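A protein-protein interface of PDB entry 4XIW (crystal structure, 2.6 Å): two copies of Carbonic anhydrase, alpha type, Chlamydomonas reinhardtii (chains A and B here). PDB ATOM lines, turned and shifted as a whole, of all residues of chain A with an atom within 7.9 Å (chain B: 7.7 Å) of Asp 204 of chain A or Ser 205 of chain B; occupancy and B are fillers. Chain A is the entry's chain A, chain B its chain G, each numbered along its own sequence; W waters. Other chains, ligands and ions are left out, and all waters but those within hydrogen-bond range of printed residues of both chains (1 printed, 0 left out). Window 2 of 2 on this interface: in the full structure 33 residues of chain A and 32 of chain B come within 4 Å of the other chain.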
ATOM      1  N   ALA A 104      30.938  -6.980 -31.434  1.00  0.00           N
ATOM      2  CA  ALA A 104      31.155  -8.417 -31.354  1.00  0.00           C
ATOM      3  C   ALA A 104      32.142  -8.878 -32.422  1.00  0.00           C
ATOM      4  O   ALA A 104      33.043  -9.649 -32.138  1.00  0.00           O
ATOM      5  CB  ALA A 104      29.819  -9.187 -31.466  1.00  0.00           C
ATOM      6  N   MET A 105      31.965  -8.447 -33.664  1.00  0.00           N
ATOM      7  CA  MET A 105      32.961  -8.780 -34.686  1.00  0.00           C
ATOM      8  C   MET A 105      33.158  -7.559 -35.550  1.00  0.00           C
ATOM      9  O   MET A 105      32.423  -6.584 -35.424  1.00  0.00           O
ATOM     10  CB  MET A 105      32.517  -9.971 -35.547  1.00  0.00           C
ATOM     11  CG  MET A 105      32.515 -11.316 -34.853  1.00  0.00           C
ATOM     12  SD  MET A 105      31.450 -12.507 -35.717  1.00  0.00           S
ATOM     13  CE  MET A 105      32.248 -12.595 -37.322  1.00  0.00           C
ATOM     14  N   GLU A 127      27.318  -6.511 -35.044  1.00  0.00           N
ATOM     15  CA  GLU A 127      26.614  -6.316 -33.795  1.00  0.00           C
ATOM     16  C   GLU A 127      25.805  -7.577 -33.518  1.00  0.00           C
ATOM     17  O   GLU A 127      25.311  -8.221 -34.459  1.00  0.00           O
ATOM     18  CB  GLU A 127      25.602  -5.214 -34.030  1.00  0.00           C
ATOM     19  CG  GLU A 127      25.625  -4.092 -33.085  1.00  0.00           C
ATOM     20  CD  GLU A 127      24.595  -3.053 -33.473  1.00  0.00           C
ATOM     21  OE1 GLU A 127      23.619  -3.431 -34.173  1.00  0.00           O
ATOM     22  OE2 GLU A 127      24.760  -1.860 -33.103  1.00  0.00           O
ATOM     23  N   PRO A 128      25.647  -7.943 -32.240  1.00  0.00           N
ATOM     24  CA  PRO A 128      24.711  -9.038 -32.003  1.00  0.00           C
ATOM     25  C   PRO A 128      23.293  -8.507 -32.050  1.00  0.00           C
ATOM     26  O   PRO A 128      23.119  -7.278 -32.131  1.00  0.00           O
ATOM     27  CB  PRO A 128      25.072  -9.522 -30.594  1.00  0.00           C
ATOM     28  CG  PRO A 128      25.659  -8.364 -29.937  1.00  0.00           C
ATOM     29  CD  PRO A 128      26.383  -7.583 -31.015  1.00  0.00           C
ATOM     30  N   GLY A 129      22.321  -9.421 -31.992  1.00  0.00           N
ATOM     31  CA  GLY A 129      20.909  -9.096 -32.025  1.00  0.00           C
ATOM     32  C   GLY A 129      20.203  -9.569 -33.285  1.00  0.00           C
ATOM     33  O   GLY A 129      18.975  -9.696 -33.317  1.00  0.00           O
ATOM     34  N   GLY A 130      20.971  -9.858 -34.322  1.00  0.00           N
ATOM     35  CA  GLY A 130      20.375 -10.076 -35.622  1.00  0.00           C
ATOM     36  C   GLY A 130      19.475 -11.287 -35.615  1.00  0.00           C
ATOM     37  O   GLY A 130      19.769 -12.251 -34.924  1.00  0.00           O
ATOM     38  N   LEU A 131      18.388 -11.235 -36.388  1.00  0.00           N
ATOM     39  CA  LEU A 131      17.452 -12.352 -36.479  1.00  0.00           C
ATOM     40  C   LEU A 131      17.606 -13.070 -37.796  1.00  0.00           C
ATOM     41  O   LEU A 131      16.920 -14.044 -38.064  1.00  0.00           O
ATOM     42  CB  LEU A 131      16.013 -11.866 -36.350  1.00  0.00           C
ATOM     43  CG  LEU A 131      15.666 -11.144 -35.052  1.00  0.00           C
ATOM     44  CD1 LEU A 131      14.262 -10.576 -35.160  1.00  0.00           C
ATOM     45  CD2 LEU A 131      15.800 -12.080 -33.851  1.00  0.00           C
ATOM     46  N   ILE A 132      18.514 -12.590 -38.624  1.00  0.00           N
ATOM     47  CA  ILE A 132      18.710 -13.172 -39.931  1.00  0.00           C
ATOM     48  C   ILE A 132      20.165 -13.491 -40.131  1.00  0.00           C
ATOM     49  O   ILE A 132      21.015 -12.606 -40.068  1.00  0.00           O
ATOM     50  CB  ILE A 132      18.196 -12.217 -41.001  1.00  0.00           C
ATOM     51  CG1 ILE A 132      16.664 -12.202 -40.950  1.00  0.00           C
ATOM     52  CG2 ILE A 132      18.698 -12.620 -42.366  1.00  0.00           C
ATOM     53  CD1 ILE A 132      15.973 -13.616 -41.178  1.00  0.00           C
ATOM     54  N   LYS A 201      23.593  -6.093 -37.974  1.00  0.00           N
ATOM     55  CA  LYS A 201      23.190  -7.085 -36.985  1.00  0.00           C
ATOM     56  C   LYS A 201      23.352  -8.448 -37.622  1.00  0.00           C
ATOM     57  O   LYS A 201      23.124  -8.621 -38.798  1.00  0.00           O
ATOM     58  CB  LYS A 201      21.762  -6.851 -36.484  1.00  0.00           C
ATOM     59  CG  LYS A 201      21.679  -5.824 -35.361  1.00  0.00           C
ATOM     60  CD  LYS A 201      20.233  -5.502 -34.936  1.00  0.00           C
ATOM     61  CE  LYS A 201      19.495  -4.677 -36.026  1.00  0.00           C
ATOM     62  NZ  LYS A 201      18.111  -4.241 -35.616  1.00  0.00           N
ATOM     63  N   VAL A 202      23.817  -9.391 -36.833  1.00  0.00           N
ATOM     64  CA  VAL A 202      24.060 -10.738 -37.268  1.00  0.00           C
ATOM     65  C   VAL A 202      23.525 -11.521 -36.073  1.00  0.00           C
ATOM     66  O   VAL A 202      23.451 -10.970 -34.955  1.00  0.00           O
ATOM     67  CB  VAL A 202      25.570 -10.945 -37.496  1.00  0.00           C
ATOM     68  CG1 VAL A 202      26.372 -10.719 -36.205  1.00  0.00           C
ATOM     69  CG2 VAL A 202      25.852 -12.304 -38.035  1.00  0.00           C
ATOM     70  N   PRO A 203      23.097 -12.773 -36.272  1.00  0.00           N
ATOM     71  CA  PRO A 203      22.629 -13.515 -35.076  1.00  0.00           C
ATOM     72  C   PRO A 203      23.719 -13.934 -34.101  1.00  0.00           C
ATOM     73  O   PRO A 203      24.816 -14.277 -34.507  1.00  0.00           O
ATOM     74  CB  PRO A 203      22.006 -14.768 -35.666  1.00  0.00           C
ATOM     75  CG  PRO A 203      21.626 -14.346 -37.074  1.00  0.00           C
ATOM     76  CD  PRO A 203      22.731 -13.453 -37.516  1.00  0.00           C
ATOM     77  N   ASP A 204      23.396 -13.934 -32.814  1.00  0.00           N
ATOM     78  CA  ASP A 204      24.354 -14.355 -31.776  1.00  0.00           C
ATOM     79  C   ASP A 204      24.948 -15.725 -32.028  1.00  0.00           C
ATOM     80  O   ASP A 204      26.150 -15.932 -31.787  1.00  0.00           O
ATOM     81  CB  ASP A 204      23.706 -14.312 -30.409  1.00  0.00           C
ATOM     82  CG  ASP A 204      23.221 -12.921 -30.054  1.00  0.00           C
ATOM     83  OD1 ASP A 204      23.168 -12.040 -30.946  1.00  0.00           O
ATOM     84  OD2 ASP A 204      22.896 -12.706 -28.884  1.00  0.00           O
ATOM     85  N   SER A 205      24.128 -16.646 -32.538  1.00  0.00           N
ATOM     86  CA  SER A 205      24.636 -17.920 -33.058  1.00  0.00           C
ATOM     87  C   SER A 205      25.922 -17.738 -33.890  1.00  0.00           C
ATOM     88  O   SER A 205      26.936 -18.387 -33.597  1.00  0.00           O
ATOM     89  CB  SER A 205      23.567 -18.651 -33.874  1.00  0.00           C
ATOM     90  OG  SER A 205      23.239 -17.961 -35.078  1.00  0.00           O
ATOM     91  N   GLN A 206      25.916 -16.825 -34.867  1.00  0.00           N
ATOM     92  CA  GLN A 206      27.045 -16.711 -35.776  1.00  0.00           C
ATOM     93  C   GLN A 206      28.282 -16.092 -35.136  1.00  0.00           C
ATOM     94  O   GLN A 206      29.415 -16.510 -35.427  1.00  0.00           O
ATOM     95  CB  GLN A 206      26.654 -15.921 -37.013  1.00  0.00           C
ATOM     96  CG  GLN A 206      25.602 -16.587 -37.864  1.00  0.00           C
ATOM     97  CD  GLN A 206      25.480 -15.953 -39.219  1.00  0.00           C
ATOM     98  OE1 GLN A 206      25.055 -14.805 -39.346  1.00  0.00           O
ATOM     99  NE2 GLN A 206      25.868 -16.694 -40.247  1.00  0.00           N
ATOM    100  N   ILE A 207      28.098 -15.097 -34.276  1.00  0.00           N
ATOM    101  CA  ILE A 207      29.247 -14.576 -33.539  1.00  0.00           C
ATOM    102  C   ILE A 207      29.900 -15.720 -32.752  1.00  0.00           C
ATOM    103  O   ILE A 207      31.130 -15.926 -32.835  1.00  0.00           O
ATOM    104  CB  ILE A 207      28.837 -13.468 -32.599  1.00  0.00           C
ATOM    105  CG1 ILE A 207      28.467 -12.239 -33.424  1.00  0.00           C
ATOM    106  CG2 ILE A 207      29.926 -13.156 -31.582  1.00  0.00           C
ATOM    107  CD1 ILE A 207      27.480 -11.351 -32.684  1.00  0.00           C
ATOM    108  N   LEU A 208      29.091 -16.502 -32.030  1.00  0.00           N
ATOM    109  CA  LEU A 208      29.663 -17.644 -31.309  1.00  0.00           C
ATOM    110  C   LEU A 208      30.301 -18.686 -32.237  1.00  0.00           C
ATOM    111  O   LEU A 208      31.387 -19.176 -31.944  1.00  0.00           O
ATOM    112  CB  LEU A 208      28.636 -18.308 -30.389  1.00  0.00           C
ATOM    113  CG  LEU A 208      28.200 -17.462 -29.180  1.00  0.00           C
ATOM    114  CD1 LEU A 208      27.067 -18.156 -28.456  1.00  0.00           C
ATOM    115  CD2 LEU A 208      29.378 -17.187 -28.270  1.00  0.00           C
ATOM    116  N   ASP A 209      29.657 -19.003 -33.353  1.00  0.00           N
ATOM    117  CA  ASP A 209      30.255 -19.914 -34.328  1.00  0.00           C
ATOM    118  C   ASP A 209      31.636 -19.455 -34.688  1.00  0.00           C
ATOM    119  O   ASP A 209      32.575 -20.261 -34.851  1.00  0.00           O
ATOM    120  CB  ASP A 209      29.437 -19.953 -35.611  1.00  0.00           C
ATOM    121  CG  ASP A 209      28.178 -20.814 -35.494  1.00  0.00           C
ATOM    122  OD1 ASP A 209      27.690 -21.002 -34.352  1.00  0.00           O
ATOM    123  OD2 ASP A 209      27.678 -21.302 -36.548  1.00  0.00           O
ATOM    124  N   PHE A 210      31.774 -18.150 -34.833  1.00  0.00           N
ATOM    125  CA  PHE A 210      33.059 -17.650 -35.264  1.00  0.00           C
ATOM    126  C   PHE A 210      34.084 -17.795 -34.172  1.00  0.00           C
ATOM    127  O   PHE A 210      35.219 -18.264 -34.409  1.00  0.00           O
ATOM    128  CB  PHE A 210      32.985 -16.201 -35.717  1.00  0.00           C
ATOM    129  CG  PHE A 210      34.281 -15.684 -36.153  1.00  0.00           C
ATOM    130  CD1 PHE A 210      34.834 -16.115 -37.334  1.00  0.00           C
ATOM    131  CD2 PHE A 210      34.984 -14.808 -35.355  1.00  0.00           C
ATOM    132  CE1 PHE A 210      36.061 -15.652 -37.737  1.00  0.00           C
ATOM    133  CE2 PHE A 210      36.206 -14.337 -35.750  1.00  0.00           C
ATOM    134  CZ  PHE A 210      36.749 -14.760 -36.946  1.00  0.00           C
ATOM    135  N   MET A 211      33.697 -17.374 -32.973  1.00  0.00           N
ATOM    136  CA  MET A 211      34.578 -17.519 -31.821  1.00  0.00           C
ATOM    137  C   MET A 211      34.990 -18.978 -31.656  1.00  0.00           C
ATOM    138  O   MET A 211      36.121 -19.277 -31.323  1.00  0.00           O
ATOM    139  CB  MET A 211      33.884 -16.997 -30.591  1.00  0.00           C
ATOM    140  CG  MET A 211      34.152 -15.540 -30.363  1.00  0.00           C
ATOM    141  SD  MET A 211      32.929 -14.861 -29.236  1.00  0.00           S
ATOM    142  CE  MET A 211      33.507 -13.164 -29.074  1.00  0.00           C
ATOM    143  N   PRO B 128      25.517 -22.958 -25.752  1.00  0.00           N
ATOM    144  CA  PRO B 128      24.551 -22.161 -26.521  1.00  0.00           C
ATOM    145  C   PRO B 128      23.446 -23.028 -27.101  1.00  0.00           C
ATOM    146  O   PRO B 128      23.675 -24.210 -27.301  1.00  0.00           O
ATOM    147  CB  PRO B 128      25.403 -21.600 -27.650  1.00  0.00           C
ATOM    148  CG  PRO B 128      26.439 -22.642 -27.869  1.00  0.00           C
ATOM    149  CD  PRO B 128      26.760 -23.185 -26.509  1.00  0.00           C
ATOM    150  N   GLY B 129      22.270 -22.459 -27.354  1.00  0.00           N
ATOM    151  CA  GLY B 129      21.151 -23.196 -27.930  1.00  0.00           C
ATOM    152  C   GLY B 129      19.873 -23.040 -27.116  1.00  0.00           C
ATOM    153  O   GLY B 129      18.814 -23.580 -27.434  1.00  0.00           O
ATOM    154  N   GLY B 130      19.957 -22.268 -26.055  1.00  0.00           N
ATOM    155  CA  GLY B 130      18.848 -22.183 -25.134  1.00  0.00           C
ATOM    156  C   GLY B 130      17.691 -21.355 -25.636  1.00  0.00           C
ATOM    157  O   GLY B 130      17.875 -20.252 -26.143  1.00  0.00           O
ATOM    158  N   LYS B 133      15.999 -17.789 -21.308  1.00  0.00           N
ATOM    159  CA  LYS B 133      17.072 -17.186 -20.539  1.00  0.00           C
ATOM    160  C   LYS B 133      17.185 -18.017 -19.260  1.00  0.00           C
ATOM    161  O   LYS B 133      16.176 -18.538 -18.772  1.00  0.00           O
ATOM    162  CB  LYS B 133      16.771 -15.717 -20.195  1.00  0.00           C
ATOM    163  CG  LYS B 133      16.518 -14.820 -21.409  1.00  0.00           C
ATOM    164  CD  LYS B 133      17.034 -13.394 -21.212  1.00  0.00           C
ATOM    165  CE  LYS B 133      16.267 -12.648 -20.119  1.00  0.00           C
ATOM    166  NZ  LYS B 133      16.940 -11.359 -19.749  1.00  0.00           N
ATOM    167  N   LEU B 137      21.484 -16.701 -13.939  1.00  0.00           N
ATOM    168  CA  LEU B 137      22.418 -16.003 -14.838  1.00  0.00           C
ATOM    169  C   LEU B 137      21.909 -14.612 -15.224  1.00  0.00           C
ATOM    170  O   LEU B 137      22.598 -13.597 -15.001  1.00  0.00           O
ATOM    171  CB  LEU B 137      22.665 -16.812 -16.117  1.00  0.00           C
ATOM    172  CG  LEU B 137      23.660 -16.160 -17.078  1.00  0.00           C
ATOM    173  CD1 LEU B 137      24.962 -15.596 -16.391  1.00  0.00           C
ATOM    174  CD2 LEU B 137      23.994 -17.170 -18.155  1.00  0.00           C
ATOM    175  N   LEU B 141      23.395 -11.016 -14.299  1.00  0.00           N
ATOM    176  CA  LEU B 141      23.749 -10.063 -15.369  1.00  0.00           C
ATOM    177  C   LEU B 141      23.104  -8.678 -15.166  1.00  0.00           C
ATOM    178  O   LEU B 141      23.816  -7.671 -15.120  1.00  0.00           O
ATOM    179  CB  LEU B 141      23.380 -10.640 -16.725  1.00  0.00           C
ATOM    180  CG  LEU B 141      24.371 -11.673 -17.286  1.00  0.00           C
ATOM    181  CD1 LEU B 141      23.779 -12.414 -18.457  1.00  0.00           C
ATOM    182  CD2 LEU B 141      25.728 -11.039 -17.684  1.00  0.00           C
ATOM    183  N   VAL B 202      21.715 -22.580 -23.092  1.00  0.00           N
ATOM    184  CA  VAL B 202      21.501 -21.188 -22.726  1.00  0.00           C
ATOM    185  C   VAL B 202      21.370 -20.355 -24.009  1.00  0.00           C
ATOM    186  O   VAL B 202      21.997 -20.649 -25.023  1.00  0.00           O
ATOM    187  CB  VAL B 202      22.635 -20.717 -21.744  1.00  0.00           C
ATOM    188  CG1 VAL B 202      22.863 -19.227 -21.739  1.00  0.00           C
ATOM    189  CG2 VAL B 202      22.298 -21.148 -20.336  1.00  0.00           C
ATOM    190  N   PRO B 203      20.503 -19.342 -23.986  1.00  0.00           N
ATOM    191  CA  PRO B 203      20.427 -18.530 -25.192  1.00  0.00           C
ATOM    192  C   PRO B 203      21.768 -17.861 -25.410  1.00  0.00           C
ATOM    193  O   PRO B 203      22.388 -17.417 -24.440  1.00  0.00           O
ATOM    194  CB  PRO B 203      19.381 -17.482 -24.835  1.00  0.00           C
ATOM    195  CG  PRO B 203      18.627 -18.035 -23.693  1.00  0.00           C
ATOM    196  CD  PRO B 203      19.608 -18.850 -22.925  1.00  0.00           C
ATOM    197  N   ASP B 204      22.199 -17.760 -26.662  1.00  0.00           N
ATOM    198  CA  ASP B 204      23.488 -17.172 -26.989  1.00  0.00           C
ATOM    199  C   ASP B 204      23.583 -15.727 -26.496  1.00  0.00           C
ATOM    200  O   ASP B 204      24.690 -15.206 -26.239  1.00  0.00           O
ATOM    201  CB  ASP B 204      23.717 -17.243 -28.489  1.00  0.00           C
ATOM    202  CG  ASP B 204      23.418 -18.626 -29.058  1.00  0.00           C
ATOM    203  OD1 ASP B 204      22.543 -19.333 -28.524  1.00  0.00           O
ATOM    204  OD2 ASP B 204      24.037 -19.008 -30.063  1.00  0.00           O
ATOM    205  N   SER B 205      22.434 -15.091 -26.308  1.00  0.00           N
ATOM    206  CA  SER B 205      22.441 -13.709 -25.899  1.00  0.00           C
ATOM    207  C   SER B 205      23.170 -13.623 -24.592  1.00  0.00           C
ATOM    208  O   SER B 205      23.973 -12.714 -24.413  1.00  0.00           O
ATOM    209  CB  SER B 205      21.027 -13.128 -25.810  1.00  0.00           C
ATOM    210  OG  SER B 205      20.426 -13.415 -24.569  1.00  0.00           O
ATOM    211  N   GLN B 206      22.934 -14.603 -23.705  1.00  0.00           N
ATOM    212  CA  GLN B 206      23.453 -14.581 -22.329  1.00  0.00           C
ATOM    213  C   GLN B 206      24.937 -14.845 -22.273  1.00  0.00           C
ATOM    214  O   GLN B 206      25.664 -14.186 -21.533  1.00  0.00           O
ATOM    215  CB  GLN B 206      22.712 -15.590 -21.452  1.00  0.00           C
ATOM    216  CG  GLN B 206      21.337 -15.106 -21.010  1.00  0.00           C
ATOM    217  CD  GLN B 206      20.679 -16.000 -19.972  1.00  0.00           C
ATOM    218  OE1 GLN B 206      20.606 -17.221 -20.140  1.00  0.00           O
ATOM    219  NE2 GLN B 206      20.169 -15.387 -18.898  1.00  0.00           N
ATOM    220  N   ILE B 207      25.398 -15.812 -23.049  1.00  0.00           N
ATOM    221  CA  ILE B 207      26.838 -16.023 -23.222  1.00  0.00           C
ATOM    222  C   ILE B 207      27.549 -14.725 -23.733  1.00  0.00           C
ATOM    223  O   ILE B 207      28.584 -14.296 -23.143  1.00  0.00           O
ATOM    224  CB  ILE B 207      27.078 -17.238 -24.155  1.00  0.00           C
ATOM    225  CG1 ILE B 207      26.608 -18.523 -23.468  1.00  0.00           C
ATOM    226  CG2 ILE B 207      28.536 -17.383 -24.518  1.00  0.00           C
ATOM    227  CD1 ILE B 207      26.444 -19.682 -24.418  1.00  0.00           C
ATOM    228  N   LEU B 208      27.005 -14.077 -24.779  1.00  0.00           N
ATOM    229  CA  LEU B 208      27.590 -12.787 -25.214  1.00  0.00           C
ATOM    230  C   LEU B 208      27.464 -11.689 -24.159  1.00  0.00           C
ATOM    231  O   LEU B 208      28.422 -10.909 -23.948  1.00  0.00           O
ATOM    232  CB  LEU B 208      27.000 -12.267 -26.523  1.00  0.00           C
ATOM    233  CG  LEU B 208      27.326 -13.049 -27.782  1.00  0.00           C
ATOM    234  CD1 LEU B 208      26.655 -12.379 -28.962  1.00  0.00           C
ATOM    235  CD2 LEU B 208      28.833 -13.190 -27.986  1.00  0.00           C
ATOM    236  N   ASP B 209      26.305 -11.619 -23.500  1.00  0.00           N
ATOM    237  CA  ASP B 209      26.137 -10.680 -22.381  1.00  0.00           C
ATOM    238  C   ASP B 209      27.225 -10.890 -21.320  1.00  0.00           C
ATOM    239  O   ASP B 209      27.818  -9.923 -20.834  1.00  0.00           O
ATOM    240  CB  ASP B 209      24.756 -10.799 -21.717  1.00  0.00           C
ATOM    241  CG  ASP B 209      23.614 -10.337 -22.625  1.00  0.00           C
ATOM    242  OD1 ASP B 209      23.873  -9.736 -23.707  1.00  0.00           O
ATOM    243  OD2 ASP B 209      22.442 -10.574 -22.243  1.00  0.00           O
ATOM    244  N   PHE B 210      27.518 -12.143 -20.974  1.00  0.00           N
ATOM    245  CA  PHE B 210      28.545 -12.383 -19.970  1.00  0.00           C
ATOM    246  C   PHE B 210      29.941 -12.011 -20.463  1.00  0.00           C
ATOM    247  O   PHE B 210      30.671 -11.303 -19.758  1.00  0.00           O
ATOM    248  CB  PHE B 210      28.537 -13.830 -19.472  1.00  0.00           C
ATOM    249  CG  PHE B 210      29.631 -14.118 -18.495  1.00  0.00           C
ATOM    250  CD1 PHE B 210      29.520 -13.712 -17.187  1.00  0.00           C
ATOM    251  CD2 PHE B 210      30.803 -14.738 -18.910  1.00  0.00           C
ATOM    252  CE1 PHE B 210      30.512 -13.945 -16.318  1.00  0.00           C
ATOM    253  CE2 PHE B 210      31.801 -14.969 -18.031  1.00  0.00           C
ATOM    254  CZ  PHE B 210      31.653 -14.578 -16.735  1.00  0.00           C
ATOM    255  N   MET B 211      30.337 -12.494 -21.644  1.00  0.00           N
ATOM    256  CA  MET B 211      31.655 -12.121 -22.185  1.00  0.00           C
ATOM    257  C   MET B 211      31.795 -10.595 -22.287  1.00  0.00           C
ATOM    258  O   MET B 211      32.906 -10.038 -22.171  1.00  0.00           O
ATOM    259  CB  MET B 211      31.850 -12.711 -23.563  1.00  0.00           C
ATOM    260  CG  MET B 211      31.819 -14.188 -23.578  1.00  0.00           C
ATOM    261  SD  MET B 211      31.980 -14.821 -25.249  1.00  0.00           S
ATOM    262  CE  MET B 211      33.751 -14.584 -25.501  1.00  0.00           C
ATOM    263  N   ARG B 212      30.659  -9.930 -22.516  1.00  0.00           N
ATOM    264  CA  ARG B 212      30.595  -8.472 -22.479  1.00  0.00           C
ATOM    265  C   ARG B 212      30.876  -7.916 -21.096  1.00  0.00           C
ATOM    266  O   ARG B 212      31.689  -6.986 -20.939  1.00  0.00           O
ATOM    267  CB  ARG B 212      29.222  -7.981 -22.945  1.00  0.00           C
ATOM    268  CG  ARG B 212      29.116  -6.467 -23.143  1.00  0.00           C
ATOM    269  CD  ARG B 212      29.736  -6.015 -24.458  1.00  0.00           C
ATOM    270  NE  ARG B 212      29.782  -4.559 -24.520  1.00  0.00           N
ATOM    271  CZ  ARG B 212      30.280  -3.859 -25.536  1.00  0.00           C
ATOM    272  NH1 ARG B 212      30.796  -4.468 -26.606  1.00  0.00           N
ATOM    273  NH2 ARG B 212      30.269  -2.542 -25.467  1.00  0.00           N
ATOM    274  N   TYR B 220      34.543  -7.739 -25.697  1.00  0.00           N
ATOM    275  CA  TYR B 220      34.179  -9.095 -25.351  1.00  0.00           C
ATOM    276  C   TYR B 220      35.488  -9.797 -24.976  1.00  0.00           C
ATOM    277  O   TYR B 220      36.512  -9.641 -25.676  1.00  0.00           O
ATOM    278  CB  TYR B 220      33.459  -9.770 -26.506  1.00  0.00           C
ATOM    279  CG  TYR B 220      32.120  -9.151 -26.832  1.00  0.00           C
ATOM    280  CD1 TYR B 220      32.015  -8.040 -27.698  1.00  0.00           C
ATOM    281  CD2 TYR B 220      30.963  -9.665 -26.292  1.00  0.00           C
ATOM    282  CE1 TYR B 220      30.800  -7.472 -27.985  1.00  0.00           C
ATOM    283  CE2 TYR B 220      29.749  -9.106 -26.587  1.00  0.00           C
ATOM    284  CZ  TYR B 220      29.677  -8.011 -27.432  1.00  0.00           C
ATOM    285  OH  TYR B 220      28.442  -7.470 -27.686  1.00  0.00           O
HETATM  286  O   HOH W   1      28.607  -5.509 -30.026  1.00  0.00           O
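The backbone NH (N) of Ser 205 of chain A lies close to the side-chain carboxylate (OD2) of Asp 204 of chain B, at 3.4 Å.
OD1 of Asp 204 of chain A sits at hydrogen-bond distance from N of Gly 129 of chain A, at 2.9 Å. The backbone NH (N) of Gly 129 of chain B sits at hydrogen-bond distance from the side-chain carboxylate (OD1) of Asp 204 of chain B, 3.3 Å away.
Pro 128 of chain A touches Leu 208 of chain B, and with the chains exchanged Leu 208 of chain A touches Pro 128 of chain B. Asp 204 of chain B touches its own counterpart, Asp 204 of chain A. Asp 204 of chain A touches Leu 208 of chain B, and with the chains exchanged Leu 208 of chain A touches Asp 204 of chain B. Ile 207 of chain A touches Leu 208 of chain B, and with the chains exchanged Leu 208 of chain A touches Ile 207 of chain B. Positions printed for both chains: 128, 129, 130, 202, 203, 204, 205, 206, 207, 208, 209, 210 and 211. Of the 12 pairs that touch across the chains among the printed residues, 10 have their exchanged pair printed and touching as well.
Of the 18 printed residues of chain B, 7 touch a printed residue of chain A.
Among the printed residues, merely in contact across the chains: Asp 204 of chain A with Ser 205 of chain B, Leu 208 of chain A with Asp 204 of chain B, Ala 104 of chain A with Tyr 220 of chain B, Asp 204 of chain A with Asp 204 of chain B, Asp 204 of chain A with Leu 208 of chain B, Pro 128 of chain A with Leu 208 of chain B, Pro 128 of chain A with Tyr 220 of chain B, Ile 207 of chain A with Leu 208 of chain B, Met 211 of chain A with Met 211 of chain B, Leu 208 of chain A with Ile 207 of chain B and Leu 208 of chain A with Pro 128 of chain B.
Of the printed residues of chain B, Ala 104 of chain A touches Tyr 220. Glu 127 of chain A touches none of the printed residues of chain B. Of the printed residues of chain B, Pro 128 of chain A touches Leu 208 and Tyr 220. Printed residues of chain B within 4 Å of Met 211 of chain A: Met 211. Gly 130 of chain B touches none of the printed residues of chain A. Of the printed residues of chain A, Ser 205 of chain B touches Asp 204. Of the printed residues of chain A, Ile 207 of chain B touches Leu 208 (3.9 Å). Printed residues of chain A within 4 Å of Leu 208 of chain B: Pro 128, Asp 204 and Ile 207.
Water W1 lies within hydrogen-bond range of the side-chain hydroxyl (OH) of Tyr 220 of chain B (3.1 Å) and the backbone NH (N) of Ala 104 of chain A (3.1 Å).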
